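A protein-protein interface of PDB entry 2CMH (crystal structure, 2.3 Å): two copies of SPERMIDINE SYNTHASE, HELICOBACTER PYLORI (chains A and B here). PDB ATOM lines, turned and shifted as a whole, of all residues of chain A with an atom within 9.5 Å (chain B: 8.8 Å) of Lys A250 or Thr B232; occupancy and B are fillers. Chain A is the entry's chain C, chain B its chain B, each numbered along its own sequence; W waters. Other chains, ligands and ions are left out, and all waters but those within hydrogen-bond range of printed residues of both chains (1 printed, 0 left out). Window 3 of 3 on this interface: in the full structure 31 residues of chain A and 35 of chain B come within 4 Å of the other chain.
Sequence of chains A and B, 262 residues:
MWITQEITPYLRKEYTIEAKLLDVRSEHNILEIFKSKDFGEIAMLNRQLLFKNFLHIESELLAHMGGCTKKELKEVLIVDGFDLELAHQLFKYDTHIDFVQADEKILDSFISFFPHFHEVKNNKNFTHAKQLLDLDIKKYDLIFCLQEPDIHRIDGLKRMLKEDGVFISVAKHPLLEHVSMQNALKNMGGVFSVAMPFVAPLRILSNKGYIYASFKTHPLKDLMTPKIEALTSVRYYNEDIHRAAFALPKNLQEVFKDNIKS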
ATOM      1  N   LEU A 175      13.633 -35.018  -8.858  1.00  0.00           N
ATOM      2  CA  LEU A 175      12.861 -35.431  -7.680  1.00  0.00           C
ATOM      3  C   LEU A 175      12.530 -36.921  -7.726  1.00  0.00           C
ATOM      4  O   LEU A 175      12.802 -37.673  -6.783  1.00  0.00           O
ATOM      5  CB  LEU A 175      11.557 -34.634  -7.594  1.00  0.00           C
ATOM      6  CG  LEU A 175      11.070 -34.191  -6.209  1.00  0.00           C
ATOM      7  CD1 LEU A 175       9.589 -33.863  -6.300  1.00  0.00           C
ATOM      8  CD2 LEU A 175      11.302 -35.264  -5.150  1.00  0.00           C
ATOM      9  N   ALA A 247      14.682 -23.670 -10.114  1.00  0.00           N
ATOM     10  CA  ALA A 247      14.177 -23.709  -8.747  1.00  0.00           C
ATOM     11  C   ALA A 247      14.207 -25.135  -8.190  1.00  0.00           C
ATOM     12  O   ALA A 247      13.864 -26.096  -8.870  1.00  0.00           O
ATOM     13  CB  ALA A 247      12.759 -23.136  -8.685  1.00  0.00           C
ATOM     14  N   LEU A 248      14.641 -25.260  -6.944  1.00  0.00           N
ATOM     15  CA  LEU A 248      14.730 -26.559  -6.298  1.00  0.00           C
ATOM     16  C   LEU A 248      14.144 -26.507  -4.892  1.00  0.00           C
ATOM     17  O   LEU A 248      14.376 -25.553  -4.140  1.00  0.00           O
ATOM     18  CB  LEU A 248      16.192 -27.024  -6.201  1.00  0.00           C
ATOM     19  CG  LEU A 248      16.861 -27.694  -7.410  1.00  0.00           C
ATOM     20  CD1 LEU A 248      18.384 -27.716  -7.235  1.00  0.00           C
ATOM     21  CD2 LEU A 248      16.303 -29.099  -7.565  1.00  0.00           C
ATOM     22  N   PRO A 249      13.342 -27.521  -4.531  1.00  0.00           N
ATOM     23  CA  PRO A 249      12.775 -27.512  -3.182  1.00  0.00           C
ATOM     24  C   PRO A 249      13.885 -27.539  -2.140  1.00  0.00           C
ATOM     25  O   PRO A 249      15.041 -27.845  -2.465  1.00  0.00           O
ATOM     26  CB  PRO A 249      11.914 -28.777  -3.154  1.00  0.00           C
ATOM     27  CG  PRO A 249      12.456 -29.614  -4.256  1.00  0.00           C
ATOM     28  CD  PRO A 249      12.758 -28.616  -5.326  1.00  0.00           C
ATOM     29  N   LYS A 250      13.531 -27.222  -0.895  1.00  0.00           N
ATOM     30  CA  LYS A 250      14.504 -27.184   0.191  1.00  0.00           C
ATOM     31  C   LYS A 250      15.353 -28.444   0.311  1.00  0.00           C
ATOM     32  O   LYS A 250      16.580 -28.378   0.222  1.00  0.00           O
ATOM     33  CB  LYS A 250      13.808 -26.894   1.531  1.00  0.00           C
ATOM     34  CG  LYS A 250      14.781 -26.548   2.650  1.00  0.00           C
ATOM     35  CD  LYS A 250      14.348 -25.293   3.378  1.00  0.00           C
ATOM     36  CE  LYS A 250      13.387 -25.600   4.510  1.00  0.00           C
ATOM     37  NZ  LYS A 250      14.071 -26.234   5.677  1.00  0.00           N
ATOM     38  N   ASN A 251      14.705 -29.589   0.498  1.00  0.00           N
ATOM     39  CA  ASN A 251      15.422 -30.844   0.647  1.00  0.00           C
ATOM     40  C   ASN A 251      16.391 -31.127  -0.502  1.00  0.00           C
ATOM     41  O   ASN A 251      17.571 -31.400  -0.264  1.00  0.00           O
ATOM     42  CB  ASN A 251      14.430 -32.010   0.834  1.00  0.00           C
ATOM     43  CG  ASN A 251      13.650 -32.350  -0.432  1.00  0.00           C
ATOM     44  OD1 ASN A 251      13.049 -31.480  -1.072  1.00  0.00           O
ATOM     45  ND2 ASN A 251      13.648 -33.629  -0.791  1.00  0.00           N
ATOM     46  N   LEU A 252      15.899 -31.053  -1.739  1.00  0.00           N
ATOM     47  CA  LEU A 252      16.717 -31.298  -2.928  1.00  0.00           C
ATOM     48  C   LEU A 252      17.964 -30.430  -2.981  1.00  0.00           C
ATOM     49  O   LEU A 252      19.023 -30.884  -3.411  1.00  0.00           O
ATOM     50  CB  LEU A 252      15.884 -31.072  -4.191  1.00  0.00           C
ATOM     51  CG  LEU A 252      15.374 -32.307  -4.935  1.00  0.00           C
ATOM     52  CD1 LEU A 252      15.056 -33.437  -3.981  1.00  0.00           C
ATOM     53  CD2 LEU A 252      14.157 -31.899  -5.752  1.00  0.00           C
ATOM     54  N   GLN A 253      17.854 -29.179  -2.549  1.00  0.00           N
ATOM     55  CA  GLN A 253      19.023 -28.313  -2.562  1.00  0.00           C
ATOM     56  C   GLN A 253      20.076 -28.925  -1.657  1.00  0.00           C
ATOM     57  O   GLN A 253      21.263 -28.904  -1.959  1.00  0.00           O
ATOM     58  CB  GLN A 253      18.669 -26.907  -2.077  1.00  0.00           C
ATOM     59  CG  GLN A 253      17.840 -26.103  -3.055  1.00  0.00           C
ATOM     60  CD  GLN A 253      17.717 -24.655  -2.630  1.00  0.00           C
ATOM     61  OE1 GLN A 253      16.978 -23.872  -3.235  1.00  0.00           O
ATOM     62  NE2 GLN A 253      18.452 -24.286  -1.584  1.00  0.00           N
ATOM     63  N   GLU A 254      19.635 -29.484  -0.543  1.00  0.00           N
ATOM     64  CA  GLU A 254      20.558 -30.106   0.389  1.00  0.00           C
ATOM     65  C   GLU A 254      21.164 -31.360  -0.219  1.00  0.00           C
ATOM     66  O   GLU A 254      22.354 -31.633  -0.049  1.00  0.00           O
ATOM     67  CB  GLU A 254      19.821 -30.474   1.673  1.00  0.00           C
ATOM     68  CG  GLU A 254      19.176 -29.297   2.340  1.00  0.00           C
ATOM     69  CD  GLU A 254      18.431 -29.697   3.570  1.00  0.00           C
ATOM     70  OE1 GLU A 254      18.065 -28.798   4.358  1.00  0.00           O
ATOM     71  OE2 GLU A 254      18.204 -30.915   3.743  1.00  0.00           O
ATOM     72  N   VAL A 255      20.327 -32.129  -0.911  1.00  0.00           N
ATOM     73  CA  VAL A 255      20.760 -33.370  -1.535  1.00  0.00           C
ATOM     74  C   VAL A 255      21.824 -33.189  -2.619  1.00  0.00           C
ATOM     75  O   VAL A 255      22.752 -33.985  -2.708  1.00  0.00           O
ATOM     76  CB  VAL A 255      19.578 -34.126  -2.176  1.00  0.00           C
ATOM     77  CG1 VAL A 255      20.060 -35.459  -2.724  1.00  0.00           C
ATOM     78  CG2 VAL A 255      18.465 -34.331  -1.166  1.00  0.00           C
ATOM     79  N   PHE A 256      21.673 -32.150  -3.438  1.00  0.00           N
ATOM     80  CA  PHE A 256      22.595 -31.876  -4.534  1.00  0.00           C
ATOM     81  C   PHE A 256      23.647 -30.818  -4.187  1.00  0.00           C
ATOM     82  O   PHE A 256      24.539 -30.528  -4.990  1.00  0.00           O
ATOM     83  CB  PHE A 256      21.812 -31.389  -5.759  1.00  0.00           C
ATOM     84  CG  PHE A 256      20.853 -32.401  -6.334  1.00  0.00           C
ATOM     85  CD1 PHE A 256      21.255 -33.708  -6.586  1.00  0.00           C
ATOM     86  CD2 PHE A 256      19.569 -32.025  -6.678  1.00  0.00           C
ATOM     87  CE1 PHE A 256      20.388 -34.618  -7.176  1.00  0.00           C
ATOM     88  CE2 PHE A 256      18.696 -32.926  -7.270  1.00  0.00           C
ATOM     89  CZ  PHE A 256      19.104 -34.222  -7.518  1.00  0.00           C
ATOM     90  N   LYS A 257      23.547 -30.252  -2.987  1.00  0.00           N
ATOM     91  CA  LYS A 257      24.454 -29.197  -2.545  1.00  0.00           C
ATOM     92  C   LYS A 257      25.854 -29.177  -3.156  1.00  0.00           C
ATOM     93  O   LYS A 257      26.175 -28.286  -3.949  1.00  0.00           O
ATOM     94  CB  LYS A 257      24.566 -29.213  -1.019  1.00  0.00           C
ATOM     95  CG  LYS A 257      25.375 -28.061  -0.427  1.00  0.00           C
ATOM     96  CD  LYS A 257      24.739 -26.700  -0.704  1.00  0.00           C
ATOM     97  CE  LYS A 257      25.303 -26.047  -1.964  1.00  0.00           C
ATOM     98  NZ  LYS A 257      24.696 -24.711  -2.257  1.00  0.00           N
ATOM     99  N   HIS B  56       3.780 -33.636   2.485  1.00  0.00           N
ATOM    100  CA  HIS B  56       4.361 -32.367   2.886  1.00  0.00           C
ATOM    101  C   HIS B  56       4.487 -31.328   1.759  1.00  0.00           C
ATOM    102  O   HIS B  56       4.379 -30.123   2.003  1.00  0.00           O
ATOM    103  CB  HIS B  56       5.729 -32.618   3.493  1.00  0.00           C
ATOM    104  CG  HIS B  56       6.696 -33.237   2.537  1.00  0.00           C
ATOM    105  ND1 HIS B  56       6.562 -34.531   2.080  1.00  0.00           N
ATOM    106  CD2 HIS B  56       7.785 -32.728   1.917  1.00  0.00           C
ATOM    107  CE1 HIS B  56       7.526 -34.790   1.216  1.00  0.00           C
ATOM    108  NE2 HIS B  56       8.282 -33.714   1.097  1.00  0.00           N
ATOM    109  N   GLU B  60       2.782 -27.860   2.772  1.00  0.00           N
ATOM    110  CA  GLU B  60       3.691 -26.752   3.059  1.00  0.00           C
ATOM    111  C   GLU B  60       3.530 -25.625   2.038  1.00  0.00           C
ATOM    112  O   GLU B  60       3.513 -24.453   2.394  1.00  0.00           O
ATOM    113  CB  GLU B  60       5.147 -27.223   3.032  1.00  0.00           C
ATOM    114  CG  GLU B  60       5.531 -28.277   4.055  1.00  0.00           C
ATOM    115  CD  GLU B  60       6.950 -28.775   3.832  1.00  0.00           C
ATOM    116  OE1 GLU B  60       7.691 -28.130   3.061  1.00  0.00           O
ATOM    117  OE2 GLU B  60       7.322 -29.801   4.426  1.00  0.00           O
ATOM    118  N   HIS B  64       2.123 -22.151   3.655  1.00  0.00           N
ATOM    119  CA  HIS B  64       3.121 -21.101   3.741  1.00  0.00           C
ATOM    120  C   HIS B  64       3.094 -20.060   2.657  1.00  0.00           C
ATOM    121  O   HIS B  64       3.631 -18.980   2.836  1.00  0.00           O
ATOM    122  CB  HIS B  64       4.481 -21.763   3.886  1.00  0.00           C
ATOM    123  CG  HIS B  64       4.535 -22.671   5.073  1.00  0.00           C
ATOM    124  ND1 HIS B  64       5.205 -23.872   5.073  1.00  0.00           N
ATOM    125  CD2 HIS B  64       3.951 -22.565   6.289  1.00  0.00           C
ATOM    126  CE1 HIS B  64       5.029 -24.470   6.238  1.00  0.00           C
ATOM    127  NE2 HIS B  64       4.271 -23.696   6.993  1.00  0.00           N
ATOM    128  N   LYS B  92       1.799 -23.869  12.408  1.00  0.00           N
ATOM    129  CA  LYS B  92       3.127 -23.367  12.706  1.00  0.00           C
ATOM    130  C   LYS B  92       2.891 -21.913  13.146  1.00  0.00           C
ATOM    131  O   LYS B  92       3.684 -21.342  13.882  1.00  0.00           O
ATOM    132  CB  LYS B  92       4.015 -23.423  11.466  1.00  0.00           C
ATOM    133  CG  LYS B  92       4.702 -24.768  11.324  1.00  0.00           C
ATOM    134  CD  LYS B  92       5.654 -24.795  10.136  1.00  0.00           C
ATOM    135  CE  LYS B  92       6.477 -26.073  10.135  1.00  0.00           C
ATOM    136  NZ  LYS B  92       5.608 -27.257   9.975  1.00  0.00           N
ATOM    137  N   PRO B 201       5.988 -26.707  -8.158  1.00  0.00           N
ATOM    138  CA  PRO B 201       7.260 -27.037  -8.804  1.00  0.00           C
ATOM    139  C   PRO B 201       7.841 -28.393  -8.401  1.00  0.00           C
ATOM    140  O   PRO B 201       7.821 -28.767  -7.228  1.00  0.00           O
ATOM    141  CB  PRO B 201       8.160 -25.875  -8.397  1.00  0.00           C
ATOM    142  CG  PRO B 201       7.209 -24.720  -8.339  1.00  0.00           C
ATOM    143  CD  PRO B 201       6.022 -25.333  -7.618  1.00  0.00           C
ATOM    144  N   LEU B 202       8.359 -29.111  -9.396  1.00  0.00           N
ATOM    145  CA  LEU B 202       8.954 -30.441  -9.247  1.00  0.00           C
ATOM    146  C   LEU B 202       7.938 -31.554  -8.962  1.00  0.00           C
ATOM    147  O   LEU B 202       8.311 -32.733  -8.856  1.00  0.00           O
ATOM    148  CB  LEU B 202      10.067 -30.442  -8.196  1.00  0.00           C
ATOM    149  CG  LEU B 202      11.378 -29.756  -8.596  1.00  0.00           C
ATOM    150  CD1 LEU B 202      11.898 -30.364  -9.893  1.00  0.00           C
ATOM    151  CD2 LEU B 202      11.159 -28.281  -8.787  1.00  0.00           C
ATOM    152  N   PRO B 226      11.569 -13.008   5.601  1.00  0.00           N
ATOM    153  CA  PRO B 226      11.902 -13.368   6.986  1.00  0.00           C
ATOM    154  C   PRO B 226      11.041 -14.530   7.457  1.00  0.00           C
ATOM    155  O   PRO B 226      11.514 -15.439   8.131  1.00  0.00           O
ATOM    156  CB  PRO B 226      11.592 -12.090   7.761  1.00  0.00           C
ATOM    157  CG  PRO B 226      12.027 -11.038   6.813  1.00  0.00           C
ATOM    158  CD  PRO B 226      11.492 -11.537   5.463  1.00  0.00           C
ATOM    159  N   LYS B 227       9.767 -14.484   7.093  1.00  0.00           N
ATOM    160  CA  LYS B 227       8.842 -15.536   7.470  1.00  0.00           C
ATOM    161  C   LYS B 227       9.214 -16.855   6.808  1.00  0.00           C
ATOM    162  O   LYS B 227       9.054 -17.924   7.403  1.00  0.00           O
ATOM    163  CB  LYS B 227       7.420 -15.130   7.098  1.00  0.00           C
ATOM    164  CG  LYS B 227       6.959 -13.910   7.875  1.00  0.00           C
ATOM    165  CD  LYS B 227       5.453 -13.785   7.894  1.00  0.00           C
ATOM    166  CE  LYS B 227       5.013 -12.666   8.825  1.00  0.00           C
ATOM    167  NZ  LYS B 227       5.454 -12.924  10.219  1.00  0.00           N
ATOM    168  N   ILE B 228       9.742 -16.771   5.587  1.00  0.00           N
ATOM    169  CA  ILE B 228      10.133 -17.963   4.852  1.00  0.00           C
ATOM    170  C   ILE B 228      11.330 -18.650   5.491  1.00  0.00           C
ATOM    171  O   ILE B 228      11.355 -19.872   5.620  1.00  0.00           O
ATOM    172  CB  ILE B 228      10.501 -17.639   3.395  1.00  0.00           C
ATOM    173  CG1 ILE B 228       9.308 -17.007   2.677  1.00  0.00           C
ATOM    174  CG2 ILE B 228      10.917 -18.924   2.668  1.00  0.00           C
ATOM    175  CD1 ILE B 228       9.602 -16.582   1.262  1.00  0.00           C
ATOM    176  N   GLU B 229      12.318 -17.855   5.893  1.00  0.00           N
ATOM    177  CA  GLU B 229      13.532 -18.399   6.492  1.00  0.00           C
ATOM    178  C   GLU B 229      13.325 -18.862   7.919  1.00  0.00           C
ATOM    179  O   GLU B 229      14.118 -19.627   8.439  1.00  0.00           O
ATOM    180  CB  GLU B 229      14.668 -17.372   6.377  1.00  0.00           C
ATOM    181  CG  GLU B 229      15.040 -17.134   4.920  1.00  0.00           C
ATOM    182  CD  GLU B 229      15.799 -15.852   4.670  1.00  0.00           C
ATOM    183  OE1 GLU B 229      16.093 -15.586   3.477  1.00  0.00           O
ATOM    184  OE2 GLU B 229      16.096 -15.122   5.643  1.00  0.00           O
ATOM    185  N   ALA B 230      12.240 -18.428   8.546  1.00  0.00           N
ATOM    186  CA  ALA B 230      11.943 -18.850   9.919  1.00  0.00           C
ATOM    187  C   ALA B 230      11.497 -20.309   9.925  1.00  0.00           C
ATOM    188  O   ALA B 230      11.611 -21.010  10.936  1.00  0.00           O
ATOM    189  CB  ALA B 230      10.849 -17.973  10.520  1.00  0.00           C
ATOM    190  N   LEU B 231      11.007 -20.764   8.776  1.00  0.00           N
ATOM    191  CA  LEU B 231      10.521 -22.134   8.609  1.00  0.00           C
ATOM    192  C   LEU B 231      11.639 -23.145   8.386  1.00  0.00           C
ATOM    193  O   LEU B 231      11.789 -23.705   7.305  1.00  0.00           O
ATOM    194  CB  LEU B 231       9.529 -22.181   7.444  1.00  0.00           C
ATOM    195  CG  LEU B 231       8.362 -21.190   7.520  1.00  0.00           C
ATOM    196  CD1 LEU B 231       7.582 -21.206   6.197  1.00  0.00           C
ATOM    197  CD2 LEU B 231       7.467 -21.564   8.700  1.00  0.00           C
ATOM    198  N   THR B 232      12.405 -23.382   9.441  1.00  0.00           N
ATOM    199  CA  THR B 232      13.532 -24.303   9.411  1.00  0.00           C
ATOM    200  C   THR B 232      13.193 -25.803   9.344  1.00  0.00           C
ATOM    201  O   THR B 232      14.041 -26.601   8.940  1.00  0.00           O
ATOM    202  CB  THR B 232      14.435 -24.072  10.642  1.00  0.00           C
ATOM    203  OG1 THR B 232      13.659 -24.221  11.833  1.00  0.00           O
ATOM    204  CG2 THR B 232      15.021 -22.676  10.623  1.00  0.00           C
ATOM    205  N   SER B 233      11.978 -26.198   9.727  1.00  0.00           N
ATOM    206  CA  SER B 233      11.639 -27.628   9.711  1.00  0.00           C
ATOM    207  C   SER B 233      10.833 -28.118   8.510  1.00  0.00           C
ATOM    208  O   SER B 233      10.517 -29.312   8.416  1.00  0.00           O
ATOM    209  CB  SER B 233      10.927 -28.029  11.007  1.00  0.00           C
ATOM    210  OG  SER B 233       9.681 -27.379  11.131  1.00  0.00           O
ATOM    211  N   VAL B 234      10.497 -27.207   7.598  1.00  0.00           N
ATOM    212  CA  VAL B 234       9.767 -27.596   6.393  1.00  0.00           C
ATOM    213  C   VAL B 234      10.780 -28.278   5.463  1.00  0.00           C
ATOM    214  O   VAL B 234      11.977 -27.967   5.503  1.00  0.00           O
ATOM    215  CB  VAL B 234       9.107 -26.359   5.707  1.00  0.00           C
ATOM    216  CG1 VAL B 234       8.184 -25.649   6.709  1.00  0.00           C
ATOM    217  CG2 VAL B 234      10.163 -25.394   5.187  1.00  0.00           C
ATOM    218  N   ARG B 235      10.318 -29.213   4.641  1.00  0.00           N
ATOM    219  CA  ARG B 235      11.223 -29.944   3.761  1.00  0.00           C
ATOM    220  C   ARG B 235      11.177 -29.585   2.284  1.00  0.00           C
ATOM    221  O   ARG B 235      12.009 -30.050   1.512  1.00  0.00           O
ATOM    222  CB  ARG B 235      10.974 -31.450   3.899  1.00  0.00           C
ATOM    223  CG  ARG B 235      11.588 -32.077   5.145  1.00  0.00           C
ATOM    224  CD  ARG B 235      12.575 -33.186   4.783  1.00  0.00           C
ATOM    225  NE  ARG B 235      11.919 -34.332   4.152  1.00  0.00           N
ATOM    226  CZ  ARG B 235      10.979 -35.074   4.734  1.00  0.00           C
ATOM    227  NH1 ARG B 235      10.575 -34.800   5.969  1.00  0.00           N
ATOM    228  NH2 ARG B 235      10.435 -36.094   4.079  1.00  0.00           N
ATOM    229  N   TYR B 236      10.218 -28.756   1.898  1.00  0.00           N
ATOM    230  CA  TYR B 236      10.056 -28.406   0.497  1.00  0.00           C
ATOM    231  C   TYR B 236      10.007 -26.915   0.206  1.00  0.00           C
ATOM    232  O   TYR B 236      10.782 -26.393  -0.590  1.00  0.00           O
ATOM    233  CB  TYR B 236       8.777 -29.091  -0.024  1.00  0.00           C
ATOM    234  CG  TYR B 236       8.260 -28.614  -1.377  1.00  0.00           C
ATOM    235  CD1 TYR B 236       7.256 -27.643  -1.458  1.00  0.00           C
ATOM    236  CD2 TYR B 236       8.758 -29.140  -2.565  1.00  0.00           C
ATOM    237  CE1 TYR B 236       6.762 -27.213  -2.684  1.00  0.00           C
ATOM    238  CE2 TYR B 236       8.272 -28.713  -3.798  1.00  0.00           C
ATOM    239  CZ  TYR B 236       7.274 -27.751  -3.853  1.00  0.00           C
ATOM    240  OH  TYR B 236       6.794 -27.331  -5.071  1.00  0.00           O
ATOM    241  N   TYR B 237       9.077 -26.243   0.872  1.00  0.00           N
ATOM    242  CA  TYR B 237       8.846 -24.827   0.677  1.00  0.00           C
ATOM    243  C   TYR B 237      10.017 -23.919   1.017  1.00  0.00           C
ATOM    244  O   TYR B 237      10.665 -24.069   2.048  1.00  0.00           O
ATOM    245  CB  TYR B 237       7.607 -24.407   1.473  1.00  0.00           C
ATOM    246  CG  TYR B 237       7.258 -22.950   1.329  1.00  0.00           C
ATOM    247  CD1 TYR B 237       6.496 -22.489   0.251  1.00  0.00           C
ATOM    248  CD2 TYR B 237       7.724 -22.022   2.249  1.00  0.00           C
ATOM    249  CE1 TYR B 237       6.211 -21.130   0.104  1.00  0.00           C
ATOM    250  CE2 TYR B 237       7.450 -20.679   2.108  1.00  0.00           C
ATOM    251  CZ  TYR B 237       6.696 -20.232   1.040  1.00  0.00           C
ATOM    252  OH  TYR B 237       6.443 -18.880   0.916  1.00  0.00           O
ATOM    253  N   ASN B 238      10.282 -22.984   0.111  1.00  0.00           N
ATOM    254  CA  ASN B 238      11.338 -21.980   0.257  1.00  0.00           C
ATOM    255  C   ASN B 238      10.985 -20.844  -0.702  1.00  0.00           C
ATOM    256  O   ASN B 238      10.010 -20.950  -1.444  1.00  0.00           O
ATOM    257  CB  ASN B 238      12.730 -22.579  -0.039  1.00  0.00           C
ATOM    258  CG  ASN B 238      12.905 -23.036  -1.483  1.00  0.00           C
ATOM    259  OD1 ASN B 238      13.849 -23.774  -1.792  1.00  0.00           O
ATOM    260  ND2 ASN B 238      12.028 -22.596  -2.367  1.00  0.00           N
ATOM    261  N   GLU B 239      11.750 -19.758  -0.691  1.00  0.00           N
ATOM    262  CA  GLU B 239      11.439 -18.639  -1.568  1.00  0.00           C
ATOM    263  C   GLU B 239      11.508 -18.998  -3.059  1.00  0.00           C
ATOM    264  O   GLU B 239      10.616 -18.658  -3.829  1.00  0.00           O
ATOM    265  CB  GLU B 239      12.364 -17.445  -1.265  1.00  0.00           C
ATOM    266  CG  GLU B 239      11.952 -16.180  -2.015  1.00  0.00           C
ATOM    267  CD  GLU B 239      12.815 -14.976  -1.702  1.00  0.00           C
ATOM    268  OE1 GLU B 239      12.739 -13.996  -2.477  1.00  0.00           O
ATOM    269  OE2 GLU B 239      13.562 -14.997  -0.691  1.00  0.00           O
ATOM    270  N   ASP B 240      12.558 -19.701  -3.463  1.00  0.00           N
ATOM    271  CA  ASP B 240      12.727 -20.070  -4.864  1.00  0.00           C
ATOM    272  C   ASP B 240      11.537 -20.831  -5.426  1.00  0.00           C
ATOM    273  O   ASP B 240      11.195 -20.664  -6.585  1.00  0.00           O
ATOM    274  CB  ASP B 240      14.015 -20.890  -5.058  1.00  0.00           C
ATOM    275  CG  ASP B 240      15.274 -20.031  -5.021  1.00  0.00           C
ATOM    276  OD1 ASP B 240      15.154 -18.793  -4.891  1.00  0.00           O
ATOM    277  OD2 ASP B 240      16.388 -20.599  -5.138  1.00  0.00           O
ATOM    278  N   ILE B 241      10.912 -21.657  -4.594  1.00  0.00           N
ATOM    279  CA  ILE B 241       9.751 -22.458  -4.989  1.00  0.00           C
ATOM    280  C   ILE B 241       8.473 -21.625  -5.014  1.00  0.00           C
ATOM    281  O   ILE B 241       7.552 -21.894  -5.788  1.00  0.00           O
ATOM    282  CB  ILE B 241       9.556 -23.655  -4.010  1.00  0.00           C
ATOM    283  CG1 ILE B 241      10.635 -24.711  -4.269  1.00  0.00           C
ATOM    284  CG2 ILE B 241       8.167 -24.251  -4.148  1.00  0.00           C
ATOM    285  CD1 ILE B 241      10.573 -25.355  -5.669  1.00  0.00           C
HETATM  286  O   HOH W   1      16.832 -25.585   7.433  1.00  0.00           O
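O of Thr B232 sits at hydrogen-bond distance from NZ of Lys A250 (3.3 Å).
The backbone carbonyl oxygen (O) of Val B234 sits at hydrogen-bond distance from the side-chain amino group (NZ) of Lys A250, at 2.7 Å.
N of Asn A251 sits at hydrogen-bond distance from O of Arg B235 (2.9 Å).
O of Tyr B236 is in hydrogen-bond range of N of Lys A250 (2.9 Å).
OD1 of Asn B238 lies close to O of Leu A248 (3.0 Å).
OE1 of Gln A253 lies close to OD1 of Asn B238.
N of Arg B235 lies within hydrogen-bond range of OE2 of Glu B60 (3.1 Å).
OE1 of Glu B60 sits at hydrogen-bond distance from N of Tyr B237, at 3.2 Å.
The backbone carbonyl oxygen (O) of His B64 lies within hydrogen-bond range of the side-chain hydroxyl (OH) of Tyr B237.
The backbone carbonyl oxygen (O) of Pro B201 is in hydrogen-bond range of the side-chain hydroxyl (OH) of Tyr B236.
The side-chain amide nitrogen (ND2) of Asn B238 sits close to the backbone NH (N) of Asp B240 (3.1 Å).
The side-chain amide oxygen (OE1) of Gln A253 lies close to the backbone carbonyl oxygen (O) of Leu A248 (3.2 Å).
O of Leu B202 touches CD1 of Leu A175, 3.1 Å away.
O of Asp B240 touches CB of Ala A247 (3.6 Å).
Leu A248 touches Ile B241 (C to CD1, 3.8 Å).
CD of Pro A249 touches CG of Leu B202, at 3.7 Å.
Tyr B236 touches Pro A249.
OD1 of Asn B238 touches C of Pro A249, 3.8 Å away.
Pro A249 touches Ile B241 (CA to CG1, 3.7 Å).
Lys A250 touches Leu B231 (CE to O, 3.7 Å).
Arg B235 touches Lys A250.
Gln A253 touches Asp B240 (OE1 to OD2, 3.8 Å).
Pro A249 touches just these residues of chain B: Leu B202 (3.7 Å), Tyr B236 (3.2 Å), Asn B238 (3.8 Å) and Ile B241 (3.7 Å).
Lys A250 touches just these residues of chain B: Leu B231, Thr B232, Val B234, Arg B235, Tyr B236, Tyr B237 and Asn B238.
Of the printed residues of chain B, Gln A253 touches Asn B238 and Asp B240.
Glu B229 touches none of the printed residues of chain A.
Of the printed residues of chain A, Leu B231 touches Lys A250.
Of chain A, only Lys A250 comes within 4 Å of Thr B232.
No residue of chain A comes within 4 Å of Ser B233.
Printed residues of chain A within 4 Å of Tyr B236: Pro A249 and Lys A250.
Of the printed residues of chain A, Tyr B237 touches Lys A250.
Printed residues of chain A within 4 Å of Asn B238: Leu A248, Pro A249, Lys A250 and Gln A253.
The nearest printed residue of chain A that does not touch Asp B240 is Leu A248 (4.8 Å).
Of the 22 printed residues of chain B, 10 touch a printed residue of chain A.
Hydrophobic or aromatic side chains of chain B that line the printed part of chain A: Leu B202, Val B234, Tyr B236 and Ile B241.
Among the printed residues, no Asp or Glu carboxylate lies within 4 Å of a Lys or Arg side-chain nitrogen of the other chain.
No position is printed for both chains.
Water W1 bridges the backbone carbonyl oxygen of Thr B232 and the side-chain amino group of Lys A250.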
